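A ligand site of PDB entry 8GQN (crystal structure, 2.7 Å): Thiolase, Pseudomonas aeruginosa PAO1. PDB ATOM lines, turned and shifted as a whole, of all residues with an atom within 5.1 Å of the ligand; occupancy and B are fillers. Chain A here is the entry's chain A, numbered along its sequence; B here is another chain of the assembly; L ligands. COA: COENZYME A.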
ATOM      1  N   CYS A  88      14.541  17.209 -24.052  1.00  0.00           N
ATOM      2  CA  CYS A  88      13.149  17.112 -23.585  1.00  0.00           C
ATOM      3  C   CYS A  88      12.958  17.993 -22.356  1.00  0.00           C
ATOM      4  O   CYS A  88      11.817  18.126 -21.919  1.00  0.00           O
ATOM      5  CB  CYS A  88      12.804  15.631 -23.377  1.00  0.00           C
ATOM      6  SG  CYS A  88      13.380  14.554 -24.723  1.00  0.00           S
ATOM      7  N   LEU A 148      15.775  12.437 -31.212  1.00  0.00           N
ATOM      8  CA  LEU A 148      15.158  11.197 -30.655  1.00  0.00           C
ATOM      9  C   LEU A 148      16.122  10.004 -30.598  1.00  0.00           C
ATOM     10  O   LEU A 148      15.652   8.915 -30.190  1.00  0.00           O
ATOM     11  CB  LEU A 148      13.926  10.852 -31.491  1.00  0.00           C
ATOM     12  CG  LEU A 148      12.633  10.647 -30.710  1.00  0.00           C
ATOM     13  CD1 LEU A 148      12.456  11.746 -29.668  1.00  0.00           C
ATOM     14  CD2 LEU A 148      11.439  10.601 -31.632  1.00  0.00           C
ATOM     15  N   MET A 157      16.235   6.788 -27.858  1.00  0.00           N
ATOM     16  CA  MET A 157      15.778   6.859 -26.441  1.00  0.00           C
ATOM     17  C   MET A 157      15.028   5.581 -26.038  1.00  0.00           C
ATOM     18  O   MET A 157      15.401   5.044 -25.011  1.00  0.00           O
ATOM     19  CB  MET A 157      14.872   8.069 -26.214  1.00  0.00           C
ATOM     20  CG  MET A 157      15.533   9.393 -26.526  1.00  0.00           C
ATOM     21  SD  MET A 157      17.074   9.725 -25.656  1.00  0.00           S
ATOM     22  CE  MET A 157      18.308   8.909 -26.684  1.00  0.00           C
ATOM     23  N   LEU A 183      -4.076   6.645 -18.654  1.00  0.00           N
ATOM     24  CA  LEU A 183      -5.177   6.852 -19.647  1.00  0.00           C
ATOM     25  C   LEU A 183      -6.506   7.041 -18.920  1.00  0.00           C
ATOM     26  O   LEU A 183      -7.307   7.924 -19.345  1.00  0.00           O
ATOM     27  CB  LEU A 183      -5.241   5.618 -20.568  1.00  0.00           C
ATOM     28  CG  LEU A 183      -6.023   5.797 -21.872  1.00  0.00           C
ATOM     29  CD1 LEU A 183      -5.383   6.869 -22.745  1.00  0.00           C
ATOM     30  CD2 LEU A 183      -6.111   4.480 -22.644  1.00  0.00           C
ATOM     31  N   GLN A 218      -4.451  12.313 -27.949  1.00  0.00           N
ATOM     32  CA  GLN A 218      -4.146  10.883 -27.695  1.00  0.00           C
ATOM     33  C   GLN A 218      -5.213  10.277 -26.772  1.00  0.00           C
ATOM     34  O   GLN A 218      -5.788   9.241 -27.079  1.00  0.00           O
ATOM     35  CB  GLN A 218      -2.726  10.717 -27.151  1.00  0.00           C
ATOM     36  CG  GLN A 218      -2.330   9.265 -26.893  1.00  0.00           C
ATOM     37  CD  GLN A 218      -2.202   8.429 -28.148  1.00  0.00           C
ATOM     38  OE1 GLN A 218      -3.136   7.725 -28.545  1.00  0.00           O
ATOM     39  NE2 GLN A 218      -1.040   8.487 -28.775  1.00  0.00           N
ATOM     40  N   THR A 221      -8.157   9.325 -29.173  1.00  0.00           N
ATOM     41  CA  THR A 221      -7.791   8.325 -30.214  1.00  0.00           C
ATOM     42  C   THR A 221      -7.118   7.096 -29.570  1.00  0.00           C
ATOM     43  O   THR A 221      -6.528   6.288 -30.323  1.00  0.00           O
ATOM     44  CB  THR A 221      -6.893   9.000 -31.272  1.00  0.00           C
ATOM     45  OG1 THR A 221      -5.929   9.812 -30.604  1.00  0.00           O
ATOM     46  CG2 THR A 221      -7.670   9.847 -32.255  1.00  0.00           C
ATOM     47  N   ALA A 222      -7.227   6.936 -28.249  1.00  0.00           N
ATOM     48  CA  ALA A 222      -6.513   5.892 -27.471  1.00  0.00           C
ATOM     49  C   ALA A 222      -7.511   4.880 -26.926  1.00  0.00           C
ATOM     50  O   ALA A 222      -8.334   5.263 -26.072  1.00  0.00           O
ATOM     51  CB  ALA A 222      -5.725   6.516 -26.353  1.00  0.00           C
ATOM     52  N   ASN A 223      -7.384   3.629 -27.377  1.00  0.00           N
ATOM     53  CA  ASN A 223      -8.272   2.484 -27.021  1.00  0.00           C
ATOM     54  C   ASN A 223      -7.619   1.676 -25.894  1.00  0.00           C
ATOM     55  O   ASN A 223      -6.568   1.027 -26.138  1.00  0.00           O
ATOM     56  CB  ASN A 223      -8.594   1.642 -28.263  1.00  0.00           C
ATOM     57  CG  ASN A 223      -9.907   0.894 -28.139  1.00  0.00           C
ATOM     58  OD1 ASN A 223     -10.400   0.663 -27.037  1.00  0.00           O
ATOM     59  ND2 ASN A 223     -10.475   0.512 -29.271  1.00  0.00           N
ATOM     60  N   LEU A 224      -8.241   1.705 -24.723  1.00  0.00           N
ATOM     61  CA  LEU A 224      -7.709   1.184 -23.436  1.00  0.00           C
ATOM     62  C   LEU A 224      -7.602  -0.352 -23.450  1.00  0.00           C
ATOM     63  O   LEU A 224      -6.675  -0.869 -22.818  1.00  0.00           O
ATOM     64  CB  LEU A 224      -8.648   1.683 -22.324  1.00  0.00           C
ATOM     65  CG  LEU A 224      -8.118   1.542 -20.903  1.00  0.00           C
ATOM     66  CD1 LEU A 224      -8.360   2.823 -20.100  1.00  0.00           C
ATOM     67  CD2 LEU A 224      -8.747   0.348 -20.206  1.00  0.00           C
ATOM     68  N   ILE A 227      -4.174  -2.109 -25.061  1.00  0.00           N
ATOM     69  CA  ILE A 227      -2.858  -1.861 -24.396  1.00  0.00           C
ATOM     70  C   ILE A 227      -2.160  -3.188 -24.101  1.00  0.00           C
ATOM     71  O   ILE A 227      -0.932  -3.266 -24.200  1.00  0.00           O
ATOM     72  CB  ILE A 227      -2.990  -1.022 -23.112  1.00  0.00           C
ATOM     73  CG1 ILE A 227      -3.318   0.443 -23.395  1.00  0.00           C
ATOM     74  CG2 ILE A 227      -1.743  -1.140 -22.245  1.00  0.00           C
ATOM     75  CD1 ILE A 227      -3.603   1.247 -22.153  1.00  0.00           C
ATOM     76  N   LEU A 230      -0.750  -4.628 -27.893  1.00  0.00           N
ATOM     77  CA  LEU A 230       0.088  -3.789 -28.802  1.00  0.00           C
ATOM     78  C   LEU A 230       1.439  -4.463 -28.995  1.00  0.00           C
ATOM     79  O   LEU A 230       1.844  -5.219 -28.093  1.00  0.00           O
ATOM     80  CB  LEU A 230       0.313  -2.398 -28.228  1.00  0.00           C
ATOM     81  CG  LEU A 230      -0.919  -1.495 -28.150  1.00  0.00           C
ATOM     82  CD1 LEU A 230      -0.560  -0.186 -27.459  1.00  0.00           C
ATOM     83  CD2 LEU A 230      -1.487  -1.236 -29.533  1.00  0.00           C
ATOM     84  N   ALA A 233       8.054  -1.644 -29.449  1.00  0.00           N
ATOM     85  CA  ALA A 233       8.422  -0.460 -30.248  1.00  0.00           C
ATOM     86  C   ALA A 233       9.926  -0.367 -30.507  1.00  0.00           C
ATOM     87  O   ALA A 233      10.293   0.300 -31.472  1.00  0.00           O
ATOM     88  CB  ALA A 233       7.913   0.764 -29.541  1.00  0.00           C
ATOM     89  N   PHE A 234      10.790  -0.961 -29.670  1.00  0.00           N
ATOM     90  CA  PHE A 234      12.257  -0.730 -29.696  1.00  0.00           C
ATOM     91  C   PHE A 234      13.058  -2.041 -29.800  1.00  0.00           C
ATOM     92  O   PHE A 234      14.269  -1.934 -30.006  1.00  0.00           O
ATOM     93  CB  PHE A 234      12.651   0.121 -28.492  1.00  0.00           C
ATOM     94  CG  PHE A 234      11.790   1.346 -28.470  1.00  0.00           C
ATOM     95  CD1 PHE A 234      11.921   2.287 -29.463  1.00  0.00           C
ATOM     96  CD2 PHE A 234      10.753   1.470 -27.568  1.00  0.00           C
ATOM     97  CE1 PHE A 234      11.086   3.388 -29.513  1.00  0.00           C
ATOM     98  CE2 PHE A 234       9.929   2.579 -27.601  1.00  0.00           C
ATOM     99  CZ  PHE A 234      10.078   3.531 -28.582  1.00  0.00           C
ATOM    100  N   THR A 241       5.890  -0.665 -25.497  1.00  0.00           N
ATOM    101  CA  THR A 241       4.929  -0.424 -26.598  1.00  0.00           C
ATOM    102  C   THR A 241       4.524   1.055 -26.620  1.00  0.00           C
ATOM    103  O   THR A 241       4.802   1.773 -25.656  1.00  0.00           O
ATOM    104  CB  THR A 241       3.650  -1.251 -26.414  1.00  0.00           C
ATOM    105  OG1 THR A 241       2.801  -0.593 -25.453  1.00  0.00           O
ATOM    106  CG2 THR A 241       3.913  -2.658 -25.952  1.00  0.00           C
ATOM    107  N   ALA A 242       3.827   1.469 -27.677  1.00  0.00           N
ATOM    108  CA  ALA A 242       3.180   2.797 -27.807  1.00  0.00           C
ATOM    109  C   ALA A 242       2.551   3.231 -26.481  1.00  0.00           C
ATOM    110  O   ALA A 242       2.709   4.399 -26.142  1.00  0.00           O
ATOM    111  CB  ALA A 242       2.130   2.734 -28.890  1.00  0.00           C
ATOM    112  N   ALA A 243       1.859   2.325 -25.802  1.00  0.00           N
ATOM    113  CA  ALA A 243       0.992   2.615 -24.641  1.00  0.00           C
ATOM    114  C   ALA A 243       1.821   3.060 -23.417  1.00  0.00           C
ATOM    115  O   ALA A 243       1.333   3.946 -22.667  1.00  0.00           O
ATOM    116  CB  ALA A 243       0.125   1.402 -24.341  1.00  0.00           C
ATOM    117  N   ALA A 245       5.216   3.937 -23.788  1.00  0.00           N
ATOM    118  CA  ALA A 245       6.157   4.936 -24.342  1.00  0.00           C
ATOM    119  C   ALA A 245       5.368   6.214 -24.609  1.00  0.00           C
ATOM    120  O   ALA A 245       4.138   6.099 -24.850  1.00  0.00           O
ATOM    121  CB  ALA A 245       6.788   4.407 -25.609  1.00  0.00           C
ATOM    122  N   SER A 246       5.972   7.394 -24.520  1.00  0.00           N
ATOM    123  CA  SER A 246       5.260   8.664 -24.792  1.00  0.00           C
ATOM    124  C   SER A 246       5.043   8.743 -26.313  1.00  0.00           C
ATOM    125  O   SER A 246       5.918   8.218 -27.045  1.00  0.00           O
ATOM    126  CB  SER A 246       5.974   9.889 -24.239  1.00  0.00           C
ATOM    127  OG  SER A 246       7.002  10.360 -25.105  1.00  0.00           O
ATOM    128  N   SER A 247       3.900   9.297 -26.748  1.00  0.00           N
ATOM    129  CA  SER A 247       3.573   9.585 -28.165  1.00  0.00           C
ATOM    130  C   SER A 247       4.334  10.834 -28.618  1.00  0.00           C
ATOM    131  O   SER A 247       4.750  11.649 -27.739  1.00  0.00           O
ATOM    132  CB  SER A 247       2.085   9.722 -28.371  1.00  0.00           C
ATOM    133  OG  SER A 247       1.545  10.706 -27.508  1.00  0.00           O
ATOM    134  N   ILE A 248       4.572  10.901 -29.933  1.00  0.00           N
ATOM    135  CA  ILE A 248       5.231  12.027 -30.673  1.00  0.00           C
ATOM    136  C   ILE A 248       4.135  13.053 -30.956  1.00  0.00           C
ATOM    137  O   ILE A 248       3.116  12.690 -31.562  1.00  0.00           O
ATOM    138  CB  ILE A 248       5.884  11.476 -31.955  1.00  0.00           C
ATOM    139  CG1 ILE A 248       7.036  10.531 -31.614  1.00  0.00           C
ATOM    140  CG2 ILE A 248       6.336  12.600 -32.876  1.00  0.00           C
ATOM    141  CD1 ILE A 248       7.436   9.603 -32.748  1.00  0.00           C
ATOM    142  N   PHE A 287      19.708   7.594 -18.807  1.00  0.00           N
ATOM    143  CA  PHE A 287      18.978   8.891 -18.685  1.00  0.00           C
ATOM    144  C   PHE A 287      17.647   8.666 -17.944  1.00  0.00           C
ATOM    145  O   PHE A 287      17.268   9.529 -17.133  1.00  0.00           O
ATOM    146  CB  PHE A 287      18.814   9.596 -20.042  1.00  0.00           C
ATOM    147  CG  PHE A 287      17.795   8.986 -20.977  1.00  0.00           C
ATOM    148  CD1 PHE A 287      18.124   7.911 -21.780  1.00  0.00           C
ATOM    149  CD2 PHE A 287      16.506   9.480 -21.039  1.00  0.00           C
ATOM    150  CE1 PHE A 287      17.180   7.332 -22.622  1.00  0.00           C
ATOM    151  CE2 PHE A 287      15.563   8.898 -21.865  1.00  0.00           C
ATOM    152  CZ  PHE A 287      15.907   7.827 -22.662  1.00  0.00           C
ATOM    153  N   ALA A 317       7.882   9.932 -20.169  1.00  0.00           N
ATOM    154  CA  ALA A 317       8.566   9.571 -21.444  1.00  0.00           C
ATOM    155  C   ALA A 317       8.281   8.097 -21.762  1.00  0.00           C
ATOM    156  O   ALA A 317       7.888   7.738 -22.896  1.00  0.00           O
ATOM    157  CB  ALA A 317      10.054   9.814 -21.336  1.00  0.00           C
ATOM    158  N   PHE A 318       8.485   7.268 -20.746  1.00  0.00           N
ATOM    159  CA  PHE A 318       8.144   5.834 -20.731  1.00  0.00           C
ATOM    160  C   PHE A 318       7.616   5.541 -19.315  1.00  0.00           C
ATOM    161  O   PHE A 318       8.209   6.070 -18.371  1.00  0.00           O
ATOM    162  CB  PHE A 318       9.380   5.025 -21.148  1.00  0.00           C
ATOM    163  CG  PHE A 318      10.127   5.498 -22.370  1.00  0.00           C
ATOM    164  CD1 PHE A 318      11.149   6.431 -22.279  1.00  0.00           C
ATOM    165  CD2 PHE A 318       9.864   4.951 -23.625  1.00  0.00           C
ATOM    166  CE1 PHE A 318      11.849   6.857 -23.400  1.00  0.00           C
ATOM    167  CE2 PHE A 318      10.580   5.360 -24.748  1.00  0.00           C
ATOM    168  CZ  PHE A 318      11.561   6.323 -24.628  1.00  0.00           C
ATOM    169  N   CYS A 343       2.348   9.331 -21.548  1.00  0.00           N
ATOM    170  CA  CYS A 343       2.048   7.999 -22.158  1.00  0.00           C
ATOM    171  C   CYS A 343       0.623   7.999 -22.731  1.00  0.00           C
ATOM    172  O   CYS A 343       0.370   7.309 -23.752  1.00  0.00           O
ATOM    173  CB  CYS A 343       2.196   6.863 -21.149  1.00  0.00           C
ATOM    174  SG  CYS A 343       3.879   6.182 -21.140  1.00  0.00           S
ATOM    175  N   ALA A 344      -0.266   8.733 -22.057  1.00  0.00           N
ATOM    176  CA  ALA A 344      -1.673   8.928 -22.453  1.00  0.00           C
ATOM    177  C   ALA A 344      -1.836  10.297 -23.174  1.00  0.00           C
ATOM    178  O   ALA A 344      -2.426  10.299 -24.247  1.00  0.00           O
ATOM    179  CB  ALA A 344      -2.535   8.786 -21.229  1.00  0.00           C
ATOM    180  N   HIS A 347       3.740  13.996 -25.720  1.00  0.00           N
ATOM    181  CA  HIS A 347       5.080  14.529 -25.352  1.00  0.00           C
ATOM    182  C   HIS A 347       5.630  15.403 -26.480  1.00  0.00           C
ATOM    183  O   HIS A 347       6.395  14.935 -27.311  1.00  0.00           O
ATOM    184  CB  HIS A 347       6.037  13.379 -25.000  1.00  0.00           C
ATOM    185  CG  HIS A 347       7.311  13.835 -24.381  1.00  0.00           C
ATOM    186  ND1 HIS A 347       7.538  15.145 -24.042  1.00  0.00           N
ATOM    187  CD2 HIS A 347       8.429  13.157 -24.015  1.00  0.00           C
ATOM    188  CE1 HIS A 347       8.742  15.272 -23.524  1.00  0.00           C
ATOM    189  NE2 HIS A 347       9.309  14.061 -23.494  1.00  0.00           N
ATOM    190  N   VAL A 349       8.237  17.465 -27.139  1.00  0.00           N
ATOM    191  CA  VAL A 349       9.602  17.474 -26.521  1.00  0.00           C
ATOM    192  C   VAL A 349      10.047  18.879 -26.079  1.00  0.00           C
ATOM    193  O   VAL A 349      10.439  19.034 -24.903  1.00  0.00           O
ATOM    194  CB  VAL A 349      10.601  16.835 -27.499  1.00  0.00           C
ATOM    195  CG1 VAL A 349      10.713  15.333 -27.307  1.00  0.00           C
ATOM    196  CG2 VAL A 349      10.265  17.153 -28.947  1.00  0.00           C
ATOM    197  N   CYS A 377      13.290  13.279 -17.115  1.00  0.00           N
ATOM    198  CA  CYS A 377      14.501  12.708 -17.725  1.00  0.00           C
ATOM    199  C   CYS A 377      14.739  13.395 -19.066  1.00  0.00           C
ATOM    200  O   CYS A 377      13.792  13.949 -19.623  1.00  0.00           O
ATOM    201  CB  CYS A 377      14.372  11.200 -17.928  1.00  0.00           C
ATOM    202  SG  CYS A 377      13.221  10.654 -19.238  1.00  0.00           S
ATOM    203  N   GLY A 379      17.416  13.215 -22.762  1.00  0.00           N
ATOM    204  CA  GLY A 379      18.393  12.470 -23.582  1.00  0.00           C
ATOM    205  C   GLY A 379      19.733  13.169 -23.493  1.00  0.00           C
ATOM    206  O   GLY A 379      19.740  14.415 -23.446  1.00  0.00           O
ATOM    207  N   ARG B 133       7.137  10.042 -43.903  1.00  0.00           N
ATOM    208  CA  ARG B 133       6.361   9.881 -42.645  1.00  0.00           C
ATOM    209  C   ARG B 133       7.280   9.960 -41.419  1.00  0.00           C
ATOM    210  O   ARG B 133       7.170  10.954 -40.642  1.00  0.00           O
ATOM    211  CB  ARG B 133       5.578   8.556 -42.640  1.00  0.00           C
ATOM    212  CG  ARG B 133       4.658   8.403 -41.443  1.00  0.00           C
ATOM    213  CD  ARG B 133       4.193   6.976 -41.264  1.00  0.00           C
ATOM    214  NE  ARG B 133       4.315   6.566 -39.878  1.00  0.00           N
ATOM    215  CZ  ARG B 133       3.505   6.928 -38.882  1.00  0.00           C
ATOM    216  NH1 ARG B 133       2.468   7.718 -39.094  1.00  0.00           N
ATOM    217  NH2 ARG B 133       3.755   6.498 -37.662  1.00  0.00           N
ATOM    218  N   MET B 134       8.135   8.943 -41.238  1.00  0.00           N
ATOM    219  CA  MET B 134       8.921   8.721 -39.996  1.00  0.00           C
ATOM    220  C   MET B 134      10.055   7.749 -40.315  1.00  0.00           C
ATOM    221  O   MET B 134       9.776   6.721 -40.963  1.00  0.00           O
ATOM    222  CB  MET B 134       8.025   8.144 -38.893  1.00  0.00           C
ATOM    223  CG  MET B 134       8.496   8.459 -37.477  1.00  0.00           C
ATOM    224  SD  MET B 134       7.495   7.617 -36.222  1.00  0.00           S
ATOM    225  CE  MET B 134       6.219   8.846 -35.904  1.00  0.00           C
HETATM  226  N1A COA L   1      -3.247   3.499 -24.744  1.00  0.00           N
HETATM  227  C2A COA L   1      -3.694   2.712 -25.735  1.00  0.00           C
HETATM  228  N3A COA L   1      -3.344   2.693 -27.013  1.00  0.00           N
HETATM  229  C4A COA L   1      -2.422   3.635 -27.264  1.00  0.00           C
HETATM  230  C5A COA L   1      -1.873   4.526 -26.366  1.00  0.00           C
HETATM  231  C6A COA L   1      -2.311   4.449 -25.024  1.00  0.00           C
HETATM  232  N6A COA L   1      -1.879   5.241 -24.049  1.00  0.00           N
HETATM  233  N7A COA L   1      -0.955   5.361 -27.007  1.00  0.00           N
HETATM  234  C8A COA L   1      -0.965   4.960 -28.259  1.00  0.00           C
HETATM  235  N9A COA L   1      -1.840   3.902 -28.471  1.00  0.00           N
HETATM  236  C1B COA L   1      -2.155   3.215 -29.702  1.00  0.00           C
HETATM  237  C2B COA L   1      -2.146   4.110 -30.938  1.00  0.00           C
HETATM  238  O2B COA L   1      -3.288   4.932 -30.851  1.00  0.00           O
HETATM  239  C3B COA L   1      -2.027   3.020 -31.999  1.00  0.00           C
HETATM  240  O3B COA L   1      -3.178   2.160 -32.121  1.00  0.00           O
HETATM  241  P3B COA L   1      -3.177   1.279 -33.508  1.00  0.00           P
HETATM  242  O7A COA L   1      -1.872   0.503 -33.570  1.00  0.00           O
HETATM  243  O8A COA L   1      -3.247   2.330 -34.623  1.00  0.00           O
HETATM  244  O9A COA L   1      -4.390   0.325 -33.533  1.00  0.00           O
HETATM  245  C4B COA L   1      -0.877   2.226 -31.391  1.00  0.00           C
HETATM  246  O4B COA L   1      -1.172   2.243 -29.978  1.00  0.00           O
HETATM  247  C5B COA L   1       0.521   2.771 -31.601  1.00  0.00           C
HETATM  248  O5B COA L   1       0.643   3.471 -32.864  1.00  0.00           O
HETATM  249  P1A COA L   1       0.869   5.055 -32.909  1.00  0.00           P
HETATM  250  O1A COA L   1       1.124   5.594 -31.550  1.00  0.00           O
HETATM  251  O2A COA L   1      -0.239   5.683 -33.687  1.00  0.00           O
HETATM  252  O3A COA L   1       2.218   5.145 -33.770  1.00  0.00           O
HETATM  253  P2A COA L   1       3.614   4.371 -33.714  1.00  0.00           P
HETATM  254  O4A COA L   1       3.326   2.928 -33.401  1.00  0.00           O
HETATM  255  O5A COA L   1       4.473   4.746 -34.872  1.00  0.00           O
HETATM  256  O6A COA L   1       4.311   5.113 -32.492  1.00  0.00           O
HETATM  257  CBP COA L   1       6.123   4.765 -30.907  1.00  0.00           C
HETATM  258  CCP COA L   1       4.719   4.361 -31.316  1.00  0.00           C
HETATM  259  CDP COA L   1       6.416   4.150 -29.530  1.00  0.00           C
HETATM  260  CEP COA L   1       7.122   4.221 -31.945  1.00  0.00           C
HETATM  261  CAP COA L   1       6.265   6.295 -30.796  1.00  0.00           C
HETATM  262  OAP COA L   1       5.287   6.764 -29.884  1.00  0.00           O
HETATM  263  C9P COA L   1       7.655   6.711 -30.333  1.00  0.00           C
HETATM  264  O9P COA L   1       8.644   6.359 -30.978  1.00  0.00           O
HETATM  265  N8P COA L   1       7.731   7.426 -29.225  1.00  0.00           N
HETATM  266  C7P COA L   1       8.817   8.358 -28.986  1.00  0.00           C
HETATM  267  C6P COA L   1       9.180   8.439 -27.561  1.00  0.00           C
HETATM  268  C5P COA L   1      10.294   9.447 -27.402  1.00  0.00           C
HETATM  269  O5P COA L   1      11.333   9.328 -28.048  1.00  0.00           O
HETATM  270  N4P COA L   1      10.120  10.452 -26.551  1.00  0.00           N
HETATM  271  C3P COA L   1      11.231  11.178 -25.952  1.00  0.00           C
HETATM  272  C2P COA L   1      11.714  10.515 -24.689  1.00  0.00           C
HETATM  273  S1P COA L   1      12.986  11.478 -23.829  1.00  0.00           S
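Residues that only touch the ligand: Leu 148, Ala 242, Ile 227, Asn 223, Gln 218, Leu 230, Thr 221, Leu 183, Ala 233, Ser 247, Ala 243, Ile 248, Ala 317, Phe 234, Phe 318, His 347 and Ala 245. Hydrophobic or aromatic side chains within 4 Å of the ligand: Leu 148, Leu 183, Ile 227, Leu 230, Ala 233, Phe 234, Ala 242, Ala 243, Ala 245, Ile 248, Ala 317, Phe 318 and His 347. 21 residues have an atom within 4 Å of the ligand: Cys 88, Leu 148, Leu 183, Gln 218, Thr 221, Asn 223, Ile 227, Leu 230, Ala 233, Phe 234, Ala 242, Ala 243, Ala 245, Ser 246, Ser 247, Ile 248, Ala 317, Phe 318, Cys 343, His 347 and Arg 133 of chain B.
A nitrogen (N8P) of the ligand lies within hydrogen-bond range of the backbone carbonyl oxygen (O) of Ser 246 (2.9 Å). OG of Ser 246 sits at hydrogen-bond distance from N4P of the ligand, 3.4 Å away. O of Cys 343 sits at hydrogen-bond distance from N6A of the ligand (3.1 Å). The side-chain sulfur (SG) of Cys 88 lies close to a sulfur (S1P) of the ligand, 3.2 Å away. The guanidinium group of Arg 133 of chain B lies within salt-bridge range of an oxygen (O5A) of the ligand (3.4 Å).
The backbone carbonyl oxygen (O) of Ala 317 sits at hydrogen-bond distance from the backbone NH (N) of Ser 246. The side-chain sulfur (SG) of Cys 343 lies close to the backbone carbonyl oxygen (O) of Ala 243, 3.7 Å away. SG of Cys 343 is in hydrogen-bond range of N of Ala 245 (3.7 Å). The backbone NH of Met 157 lies within hydrogen-bond range of the backbone carbonyl oxygen of Leu 148, 3.2 Å away. The backbone carbonyl oxygen (O) of Ser 247 is in hydrogen-bond range of the backbone NH (N) of His 347 (3.3 Å). The backbone NH (N) of Ala 243 lies close to the side-chain hydroxyl (OG1) of Thr 241 (3.1 Å).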
